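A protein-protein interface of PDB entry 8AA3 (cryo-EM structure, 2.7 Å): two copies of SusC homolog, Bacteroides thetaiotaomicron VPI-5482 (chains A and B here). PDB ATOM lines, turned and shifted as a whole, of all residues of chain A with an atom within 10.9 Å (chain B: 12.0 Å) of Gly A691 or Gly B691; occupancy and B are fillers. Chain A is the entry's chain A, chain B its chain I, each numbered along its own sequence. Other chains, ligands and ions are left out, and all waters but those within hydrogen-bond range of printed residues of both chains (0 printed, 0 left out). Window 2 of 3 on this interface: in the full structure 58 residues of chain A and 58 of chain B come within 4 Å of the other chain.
Hydrophobic or aromatic side chains of chain B within 4 Å of the printed part of chain A: Val B693.
Hydrophobic or aromatic side chains of chain A within 4 Å of the printed part of chain B: Tyr A668 and Val A693.
Thr A567 touches Val B693, and with the chains exchanged Val A693 touches Thr B567.
Gly A691 touches its own counterpart, Gly B691.
15 positions are printed for both chains.
Of the 6 pairs that touch across the chains among the printed residues, 3 have their exchanged pair printed and touching as well.
Of the printed residues of chain B, Thr A567 touches Val B693 (3.7 Å).
Printed residues of chain B within 4 Å of Tyr A668: Ser B565.
Printed residues of chain B within 4 Å of Gly A691: Gly B691.
Printed residues of chain A within 4 Å of Thr B567: Val A693 (3.7 Å).
No residue of chain A comes within 4 Å of Gly B690.
Gly B691 touches just one residue of chain A: Gly A691 (3.5 Å).
No residue of chain A comes within 4 Å of Gly B692.
Of the printed residues of chain A, Val B693 touches Thr A567.
Among the printed residues, merely in contact across the chains: Thr A567 with Val B693 (3.7 Å), Tyr A668 with Ser B565 (3.9 Å), Gly A691 with Gly B691 (3.5 Å), Val A693 with Asp B550 (3.8 Å), Val A693 with Ser B565 (3.5 Å) and Val A693 with Thr B567 (3.7 Å).
The side-chain hydroxyl (OG) of Ser B565 sits at hydrogen-bond distance from the backbone carbonyl oxygen (O) of Asp B550.
N of Leu A694 lies within hydrogen-bond range of OH of Tyr A668.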
ATOM      1  N   THR A 567      24.579 -19.737 -10.627  1.00  0.00           N
ATOM      2  CA  THR A 567      24.091 -21.106 -10.548  1.00  0.00           C
ATOM      3  C   THR A 567      25.225 -22.050 -10.167  1.00  0.00           C
ATOM      4  O   THR A 567      26.327 -21.969 -10.717  1.00  0.00           O
ATOM      5  CB  THR A 567      23.477 -21.527 -11.884  1.00  0.00           C
ATOM      6  OG1 THR A 567      22.421 -20.623 -12.233  1.00  0.00           O
ATOM      7  CG2 THR A 567      22.915 -22.939 -11.797  1.00  0.00           C
ATOM      8  N   TYR A 668      19.857 -35.542 -15.500  1.00  0.00           N
ATOM      9  CA  TYR A 668      19.019 -34.346 -15.497  1.00  0.00           C
ATOM     10  C   TYR A 668      19.443 -33.372 -16.588  1.00  0.00           C
ATOM     11  O   TYR A 668      18.595 -32.747 -17.237  1.00  0.00           O
ATOM     12  CB  TYR A 668      19.072 -33.676 -14.122  1.00  0.00           C
ATOM     13  CG  TYR A 668      18.092 -32.537 -13.948  1.00  0.00           C
ATOM     14  CD1 TYR A 668      16.799 -32.772 -13.501  1.00  0.00           C
ATOM     15  CD2 TYR A 668      18.462 -31.227 -14.223  1.00  0.00           C
ATOM     16  CE1 TYR A 668      15.900 -31.735 -13.337  1.00  0.00           C
ATOM     17  CE2 TYR A 668      17.571 -30.184 -14.061  1.00  0.00           C
ATOM     18  CZ  TYR A 668      16.292 -30.443 -13.618  1.00  0.00           C
ATOM     19  OH  TYR A 668      15.401 -29.406 -13.457  1.00  0.00           O
ATOM     20  N   TYR A 683      12.274 -31.799 -18.822  1.00  0.00           N
ATOM     21  CA  TYR A 683      11.361 -31.141 -19.745  1.00  0.00           C
ATOM     22  C   TYR A 683      10.398 -30.255 -18.974  1.00  0.00           C
ATOM     23  O   TYR A 683       9.899 -30.639 -17.912  1.00  0.00           O
ATOM     24  CB  TYR A 683      10.578 -32.163 -20.577  1.00  0.00           C
ATOM     25  CG  TYR A 683       9.863 -31.563 -21.766  1.00  0.00           C
ATOM     26  CD1 TYR A 683      10.570 -31.143 -22.885  1.00  0.00           C
ATOM     27  CD2 TYR A 683       8.483 -31.413 -21.770  1.00  0.00           C
ATOM     28  CE1 TYR A 683       9.924 -30.593 -23.976  1.00  0.00           C
ATOM     29  CE2 TYR A 683       7.826 -30.865 -22.857  1.00  0.00           C
ATOM     30  CZ  TYR A 683       8.551 -30.456 -23.956  1.00  0.00           C
ATOM     31  OH  TYR A 683       7.904 -29.910 -25.039  1.00  0.00           O
ATOM     32  N   ASP A 684      10.138 -29.065 -19.517  1.00  0.00           N
ATOM     33  CA  ASP A 684       9.174 -28.132 -18.935  1.00  0.00           C
ATOM     34  C   ASP A 684       7.783 -28.530 -19.419  1.00  0.00           C
ATOM     35  O   ASP A 684       7.207 -27.936 -20.333  1.00  0.00           O
ATOM     36  CB  ASP A 684       9.519 -26.697 -19.312  1.00  0.00           C
ATOM     37  CG  ASP A 684       8.664 -25.679 -18.583  1.00  0.00           C
ATOM     38  OD1 ASP A 684       7.945 -26.067 -17.638  1.00  0.00           O
ATOM     39  OD2 ASP A 684       8.711 -24.487 -18.955  1.00  0.00           O
ATOM     40  N   ILE A 685       7.237 -29.569 -18.783  1.00  0.00           N
ATOM     41  CA  ILE A 685       5.941 -30.095 -19.199  1.00  0.00           C
ATOM     42  C   ILE A 685       4.834 -29.075 -18.955  1.00  0.00           C
ATOM     43  O   ILE A 685       3.830 -29.055 -19.679  1.00  0.00           O
ATOM     44  CB  ILE A 685       5.657 -31.435 -18.492  1.00  0.00           C
ATOM     45  CG1 ILE A 685       4.510 -32.175 -19.184  1.00  0.00           C
ATOM     46  CG2 ILE A 685       5.360 -31.226 -17.011  1.00  0.00           C
ATOM     47  CD1 ILE A 685       4.843 -32.634 -20.586  1.00  0.00           C
ATOM     48  N   THR A 686       4.992 -28.213 -17.949  1.00  0.00           N
ATOM     49  CA  THR A 686       3.982 -27.191 -17.688  1.00  0.00           C
ATOM     50  C   THR A 686       4.016 -26.096 -18.747  1.00  0.00           C
ATOM     51  O   THR A 686       2.967 -25.573 -19.141  1.00  0.00           O
ATOM     52  CB  THR A 686       4.181 -26.596 -16.294  1.00  0.00           C
ATOM     53  OG1 THR A 686       5.474 -25.980 -16.216  1.00  0.00           O
ATOM     54  CG2 THR A 686       4.076 -27.679 -15.232  1.00  0.00           C
ATOM     55  N   GLY A 687       5.207 -25.737 -19.218  1.00  0.00           N
ATOM     56  CA  GLY A 687       5.343 -24.693 -20.215  1.00  0.00           C
ATOM     57  C   GLY A 687       5.483 -23.312 -19.610  1.00  0.00           C
ATOM     58  O   GLY A 687       4.936 -22.337 -20.135  1.00  0.00           O
ATOM     59  N   SER A 688       6.215 -23.216 -18.502  1.00  0.00           N
ATOM     60  CA  SER A 688       6.421 -21.958 -17.800  1.00  0.00           C
ATOM     61  C   SER A 688       7.779 -21.334 -18.093  1.00  0.00           C
ATOM     62  O   SER A 688       8.181 -20.396 -17.396  1.00  0.00           O
ATOM     63  CB  SER A 688       6.257 -22.163 -16.292  1.00  0.00           C
ATOM     64  OG  SER A 688       7.174 -23.130 -15.807  1.00  0.00           O
ATOM     65  N   ASN A 689       8.490 -21.833 -19.108  1.00  0.00           N
ATOM     66  CA  ASN A 689       9.815 -21.328 -19.478  1.00  0.00           C
ATOM     67  C   ASN A 689      10.787 -21.392 -18.301  1.00  0.00           C
ATOM     68  O   ASN A 689      11.553 -20.460 -18.050  1.00  0.00           O
ATOM     69  CB  ASN A 689       9.732 -19.905 -20.038  1.00  0.00           C
ATOM     70  CG  ASN A 689       9.083 -19.855 -21.406  1.00  0.00           C
ATOM     71  OD1 ASN A 689       8.003 -19.288 -21.574  1.00  0.00           O
ATOM     72  ND2 ASN A 689       9.743 -20.446 -22.395  1.00  0.00           N
ATOM     73  N   GLY A 690      10.755 -22.506 -17.572  1.00  0.00           N
ATOM     74  CA  GLY A 690      11.662 -22.685 -16.456  1.00  0.00           C
ATOM     75  C   GLY A 690      11.204 -21.947 -15.208  1.00  0.00           C
ATOM     76  O   GLY A 690      10.014 -21.726 -14.983  1.00  0.00           O
ATOM     77  N   GLY A 691      12.177 -21.564 -14.388  1.00  0.00           N
ATOM     78  CA  GLY A 691      11.909 -20.905 -13.129  1.00  0.00           C
ATOM     79  C   GLY A 691      11.929 -21.801 -11.912  1.00  0.00           C
ATOM     80  O   GLY A 691      11.586 -21.335 -10.819  1.00  0.00           O
ATOM     81  N   GLY A 692      12.317 -23.060 -12.063  1.00  0.00           N
ATOM     82  CA  GLY A 692      12.348 -23.967 -10.933  1.00  0.00           C
ATOM     83  C   GLY A 692      12.924 -25.303 -11.341  1.00  0.00           C
ATOM     84  O   GLY A 692      13.536 -25.441 -12.403  1.00  0.00           O
ATOM     85  N   VAL A 693      12.718 -26.294 -10.478  1.00  0.00           N
ATOM     86  CA  VAL A 693      13.204 -27.647 -10.729  1.00  0.00           C
ATOM     87  C   VAL A 693      12.215 -28.339 -11.662  1.00  0.00           C
ATOM     88  O   VAL A 693      11.066 -28.588 -11.291  1.00  0.00           O
ATOM     89  CB  VAL A 693      13.382 -28.433  -9.426  1.00  0.00           C
ATOM     90  CG1 VAL A 693      13.675 -29.897  -9.724  1.00  0.00           C
ATOM     91  CG2 VAL A 693      14.493 -27.822  -8.586  1.00  0.00           C
ATOM     92  N   LEU A 694      12.662 -28.650 -12.876  1.00  0.00           N
ATOM     93  CA  LEU A 694      11.813 -29.320 -13.845  1.00  0.00           C
ATOM     94  C   LEU A 694      11.683 -30.804 -13.510  1.00  0.00           C
ATOM     95  O   LEU A 694      12.577 -31.389 -12.890  1.00  0.00           O
ATOM     96  CB  LEU A 694      12.381 -29.161 -15.252  1.00  0.00           C
ATOM     97  CG  LEU A 694      12.284 -27.772 -15.886  1.00  0.00           C
ATOM     98  CD1 LEU A 694      12.625 -27.840 -17.366  1.00  0.00           C
ATOM     99  CD2 LEU A 694      10.900 -27.177 -15.677  1.00  0.00           C
ATOM    100  N   PRO A 695      10.572 -31.432 -13.896  1.00  0.00           N
ATOM    101  CA  PRO A 695      10.449 -32.883 -13.711  1.00  0.00           C
ATOM    102  C   PRO A 695      11.525 -33.627 -14.488  1.00  0.00           C
ATOM    103  O   PRO A 695      11.920 -33.220 -15.582  1.00  0.00           O
ATOM    104  CB  PRO A 695       9.047 -33.193 -14.246  1.00  0.00           C
ATOM    105  CG  PRO A 695       8.311 -31.896 -14.171  1.00  0.00           C
ATOM    106  CD  PRO A 695       9.335 -30.832 -14.421  1.00  0.00           C
ATOM    107  N   ASP B 550      16.804 -34.266  -4.238  1.00  0.00           N
ATOM    108  CA  ASP B 550      15.795 -34.943  -5.055  1.00  0.00           C
ATOM    109  C   ASP B 550      16.293 -36.304  -5.556  1.00  0.00           C
ATOM    110  O   ASP B 550      16.484 -36.539  -6.751  1.00  0.00           O
ATOM    111  CB  ASP B 550      15.346 -34.051  -6.220  1.00  0.00           C
ATOM    112  CG  ASP B 550      14.649 -32.789  -5.749  1.00  0.00           C
ATOM    113  OD1 ASP B 550      14.411 -32.659  -4.530  1.00  0.00           O
ATOM    114  OD2 ASP B 550      14.328 -31.931  -6.598  1.00  0.00           O
ATOM    115  N   SER B 565      18.473 -34.984  -8.838  1.00  0.00           N
ATOM    116  CA  SER B 565      17.599 -34.295  -9.780  1.00  0.00           C
ATOM    117  C   SER B 565      17.018 -33.024  -9.173  1.00  0.00           C
ATOM    118  O   SER B 565      15.913 -32.607  -9.537  1.00  0.00           O
ATOM    119  CB  SER B 565      16.468 -35.213 -10.252  1.00  0.00           C
ATOM    120  OG  SER B 565      15.746 -35.738  -9.152  1.00  0.00           O
ATOM    121  N   GLY B 566      17.745 -32.397  -8.252  1.00  0.00           N
ATOM    122  CA  GLY B 566      17.260 -31.195  -7.603  1.00  0.00           C
ATOM    123  C   GLY B 566      18.250 -30.050  -7.623  1.00  0.00           C
ATOM    124  O   GLY B 566      19.204 -30.056  -8.406  1.00  0.00           O
ATOM    125  N   THR B 567      18.025 -29.056  -6.768  1.00  0.00           N
ATOM    126  CA  THR B 567      18.918 -27.907  -6.697  1.00  0.00           C
ATOM    127  C   THR B 567      20.280 -28.331  -6.162  1.00  0.00           C
ATOM    128  O   THR B 567      20.370 -29.065  -5.173  1.00  0.00           O
ATOM    129  CB  THR B 567      18.314 -26.819  -5.810  1.00  0.00           C
ATOM    130  OG1 THR B 567      17.029 -26.442  -6.321  1.00  0.00           O
ATOM    131  CG2 THR B 567      19.216 -25.593  -5.773  1.00  0.00           C
ATOM    132  N   TYR B 668      25.733 -14.884  -0.800  1.00  0.00           N
ATOM    133  CA  TYR B 668      24.492 -14.942  -1.567  1.00  0.00           C
ATOM    134  C   TYR B 668      23.356 -15.526  -0.738  1.00  0.00           C
ATOM    135  O   TYR B 668      22.214 -15.060  -0.821  1.00  0.00           O
ATOM    136  CB  TYR B 668      24.706 -15.757  -2.844  1.00  0.00           C
ATOM    137  CG  TYR B 668      23.539 -15.722  -3.806  1.00  0.00           C
ATOM    138  CD1 TYR B 668      23.439 -14.724  -4.768  1.00  0.00           C
ATOM    139  CD2 TYR B 668      22.545 -16.691  -3.762  1.00  0.00           C
ATOM    140  CE1 TYR B 668      22.378 -14.688  -5.651  1.00  0.00           C
ATOM    141  CE2 TYR B 668      21.481 -16.662  -4.642  1.00  0.00           C
ATOM    142  CZ  TYR B 668      21.402 -15.659  -5.585  1.00  0.00           C
ATOM    143  OH  TYR B 668      20.343 -15.628  -6.463  1.00  0.00           O
ATOM    144  N   ALA B 682      20.772 -11.451  -1.171  1.00  0.00           N
ATOM    145  CA  ALA B 682      20.044 -11.775  -2.395  1.00  0.00           C
ATOM    146  C   ALA B 682      18.611 -11.303  -2.221  1.00  0.00           C
ATOM    147  O   ALA B 682      17.899 -11.806  -1.346  1.00  0.00           O
ATOM    148  CB  ALA B 682      20.092 -13.274  -2.688  1.00  0.00           C
ATOM    149  N   TYR B 683      18.190 -10.343  -3.041  1.00  0.00           N
ATOM    150  CA  TYR B 683      16.856  -9.771  -2.943  1.00  0.00           C
ATOM    151  C   TYR B 683      16.194  -9.768  -4.312  1.00  0.00           C
ATOM    152  O   TYR B 683      16.835  -9.461  -5.322  1.00  0.00           O
ATOM    153  CB  TYR B 683      16.900  -8.344  -2.383  1.00  0.00           C
ATOM    154  CG  TYR B 683      15.552  -7.814  -1.952  1.00  0.00           C
ATOM    155  CD1 TYR B 683      14.936  -8.284  -0.799  1.00  0.00           C
ATOM    156  CD2 TYR B 683      14.892  -6.846  -2.699  1.00  0.00           C
ATOM    157  CE1 TYR B 683      13.704  -7.804  -0.400  1.00  0.00           C
ATOM    158  CE2 TYR B 683      13.659  -6.360  -2.307  1.00  0.00           C
ATOM    159  CZ  TYR B 683      13.069  -6.842  -1.157  1.00  0.00           C
ATOM    160  OH  TYR B 683      11.842  -6.361  -0.763  1.00  0.00           O
ATOM    161  N   ASP B 684      14.906 -10.109  -4.337  1.00  0.00           N
ATOM    162  CA  ASP B 684      14.113 -10.080  -5.566  1.00  0.00           C
ATOM    163  C   ASP B 684      13.621  -8.651  -5.774  1.00  0.00           C
ATOM    164  O   ASP B 684      12.472  -8.299  -5.494  1.00  0.00           O
ATOM    165  CB  ASP B 684      12.960 -11.073  -5.485  1.00  0.00           C
ATOM    166  CG  ASP B 684      12.220 -11.217  -6.801  1.00  0.00           C
ATOM    167  OD1 ASP B 684      12.717 -10.708  -7.827  1.00  0.00           O
ATOM    168  OD2 ASP B 684      11.139 -11.842  -6.809  1.00  0.00           O
ATOM    169  N   ILE B 685      14.526  -7.808  -6.278  1.00  0.00           N
ATOM    170  CA  ILE B 685      14.203  -6.396  -6.457  1.00  0.00           C
ATOM    171  C   ILE B 685      13.113  -6.213  -7.508  1.00  0.00           C
ATOM    172  O   ILE B 685      12.333  -5.256  -7.441  1.00  0.00           O
ATOM    173  CB  ILE B 685      15.477  -5.598  -6.801  1.00  0.00           C
ATOM    174  CG1 ILE B 685      15.235  -4.098  -6.620  1.00  0.00           C
ATOM    175  CG2 ILE B 685      15.957  -5.908  -8.213  1.00  0.00           C
ATOM    176  CD1 ILE B 685      14.998  -3.690  -5.182  1.00  0.00           C
ATOM    177  N   THR B 686      13.033  -7.118  -8.487  1.00  0.00           N
ATOM    178  CA  THR B 686      11.990  -7.015  -9.503  1.00  0.00           C
ATOM    179  C   THR B 686      10.625  -7.381  -8.933  1.00  0.00           C
ATOM    180  O   THR B 686       9.610  -6.774  -9.297  1.00  0.00           O
ATOM    181  CB  THR B 686      12.327  -7.906 -10.698  1.00  0.00           C
ATOM    182  OG1 THR B 686      12.407  -9.272 -10.271  1.00  0.00           O
ATOM    183  CG2 THR B 686      13.657  -7.493 -11.311  1.00  0.00           C
ATOM    184  N   GLY B 687      10.578  -8.367  -8.040  1.00  0.00           N
ATOM    185  CA  GLY B 687       9.325  -8.798  -7.455  1.00  0.00           C
ATOM    186  C   GLY B 687       8.634  -9.879  -8.261  1.00  0.00           C
ATOM    187  O   GLY B 687       7.407  -9.882  -8.388  1.00  0.00           O
ATOM    188  N   SER B 688       9.417 -10.804  -8.812  1.00  0.00           N
ATOM    189  CA  SER B 688       8.898 -11.891  -9.630  1.00  0.00           C
ATOM    190  C   SER B 688       8.806 -13.209  -8.869  1.00  0.00           C
ATOM    191  O   SER B 688       8.605 -14.256  -9.493  1.00  0.00           O
ATOM    192  CB  SER B 688       9.764 -12.069 -10.879  1.00  0.00           C
ATOM    193  OG  SER B 688      11.109 -12.343 -10.532  1.00  0.00           O
ATOM    194  N   ASN B 689       8.946 -13.176  -7.542  1.00  0.00           N
ATOM    195  CA  ASN B 689       8.893 -14.377  -6.705  1.00  0.00           C
ATOM    196  C   ASN B 689       9.928 -15.411  -7.144  1.00  0.00           C
ATOM    197  O   ASN B 689       9.646 -16.609  -7.217  1.00  0.00           O
ATOM    198  CB  ASN B 689       7.488 -14.985  -6.692  1.00  0.00           C
ATOM    199  CG  ASN B 689       6.493 -14.135  -5.928  1.00  0.00           C
ATOM    200  OD1 ASN B 689       5.550 -13.593  -6.505  1.00  0.00           O
ATOM    201  ND2 ASN B 689       6.698 -14.015  -4.621  1.00  0.00           N
ATOM    202  N   GLY B 690      11.138 -14.943  -7.440  1.00  0.00           N
ATOM    203  CA  GLY B 690      12.205 -15.846  -7.830  1.00  0.00           C
ATOM    204  C   GLY B 690      12.101 -16.276  -9.284  1.00  0.00           C
ATOM    205  O   GLY B 690      11.578 -15.559 -10.140  1.00  0.00           O
ATOM    206  N   GLY B 691      12.612 -17.471  -9.559  1.00  0.00           N
ATOM    207  CA  GLY B 691      12.647 -18.003 -10.903  1.00  0.00           C
ATOM    208  C   GLY B 691      13.963 -17.840 -11.629  1.00  0.00           C
ATOM    209  O   GLY B 691      14.033 -18.156 -12.822  1.00  0.00           O
ATOM    210  N   GLY B 692      14.999 -17.360 -10.955  1.00  0.00           N
ATOM    211  CA  GLY B 692      16.283 -17.173 -11.602  1.00  0.00           C
ATOM    212  C   GLY B 692      17.320 -16.720 -10.600  1.00  0.00           C
ATOM    213  O   GLY B 692      17.122 -16.809  -9.386  1.00  0.00           O
ATOM    214  N   VAL B 693      18.438 -16.229 -11.129  1.00  0.00           N
ATOM    215  CA  VAL B 693      19.533 -15.742 -10.296  1.00  0.00           C
ATOM    216  C   VAL B 693      19.195 -14.322  -9.852  1.00  0.00           C
ATOM    217  O   VAL B 693      19.121 -13.404 -10.672  1.00  0.00           O
ATOM    218  CB  VAL B 693      20.871 -15.786 -11.042  1.00  0.00           C
ATOM    219  CG1 VAL B 693      21.950 -15.074 -10.239  1.00  0.00           C
ATOM    220  CG2 VAL B 693      21.272 -17.225 -11.326  1.00  0.00           C
ATOM    221  N   LEU B 694      18.984 -14.142  -8.550  1.00  0.00           N
ATOM    222  CA  LEU B 694      18.666 -12.831  -8.010  1.00  0.00           C
ATOM    223  C   LEU B 694      19.919 -11.962  -7.933  1.00  0.00           C
ATOM    224  O   LEU B 694      21.034 -12.479  -7.814  1.00  0.00           O
ATOM    225  CB  LEU B 694      18.047 -12.962  -6.622  1.00  0.00           C
ATOM    226  CG  LEU B 694      16.624 -13.519  -6.548  1.00  0.00           C
ATOM    227  CD1 LEU B 694      16.052 -13.324  -5.152  1.00  0.00           C
ATOM    228  CD2 LEU B 694      15.732 -12.868  -7.593  1.00  0.00           C
ATOM    229  N   PRO B 695      19.764 -10.641  -8.012  1.00  0.00           N
ATOM    230  CA  PRO B 695      20.917  -9.754  -7.820  1.00  0.00           C
ATOM    231  C   PRO B 695      21.510  -9.924  -6.429  1.00  0.00           C
ATOM    232  O   PRO B 695      20.794 -10.156  -5.452  1.00  0.00           O
ATOM    233  CB  PRO B 695      20.327  -8.353  -8.017  1.00  0.00           C
ATOM    234  CG  PRO B 695      19.087  -8.569  -8.819  1.00  0.00           C
ATOM    235  CD  PRO B 695      18.549  -9.899  -8.389  1.00  0.00           C
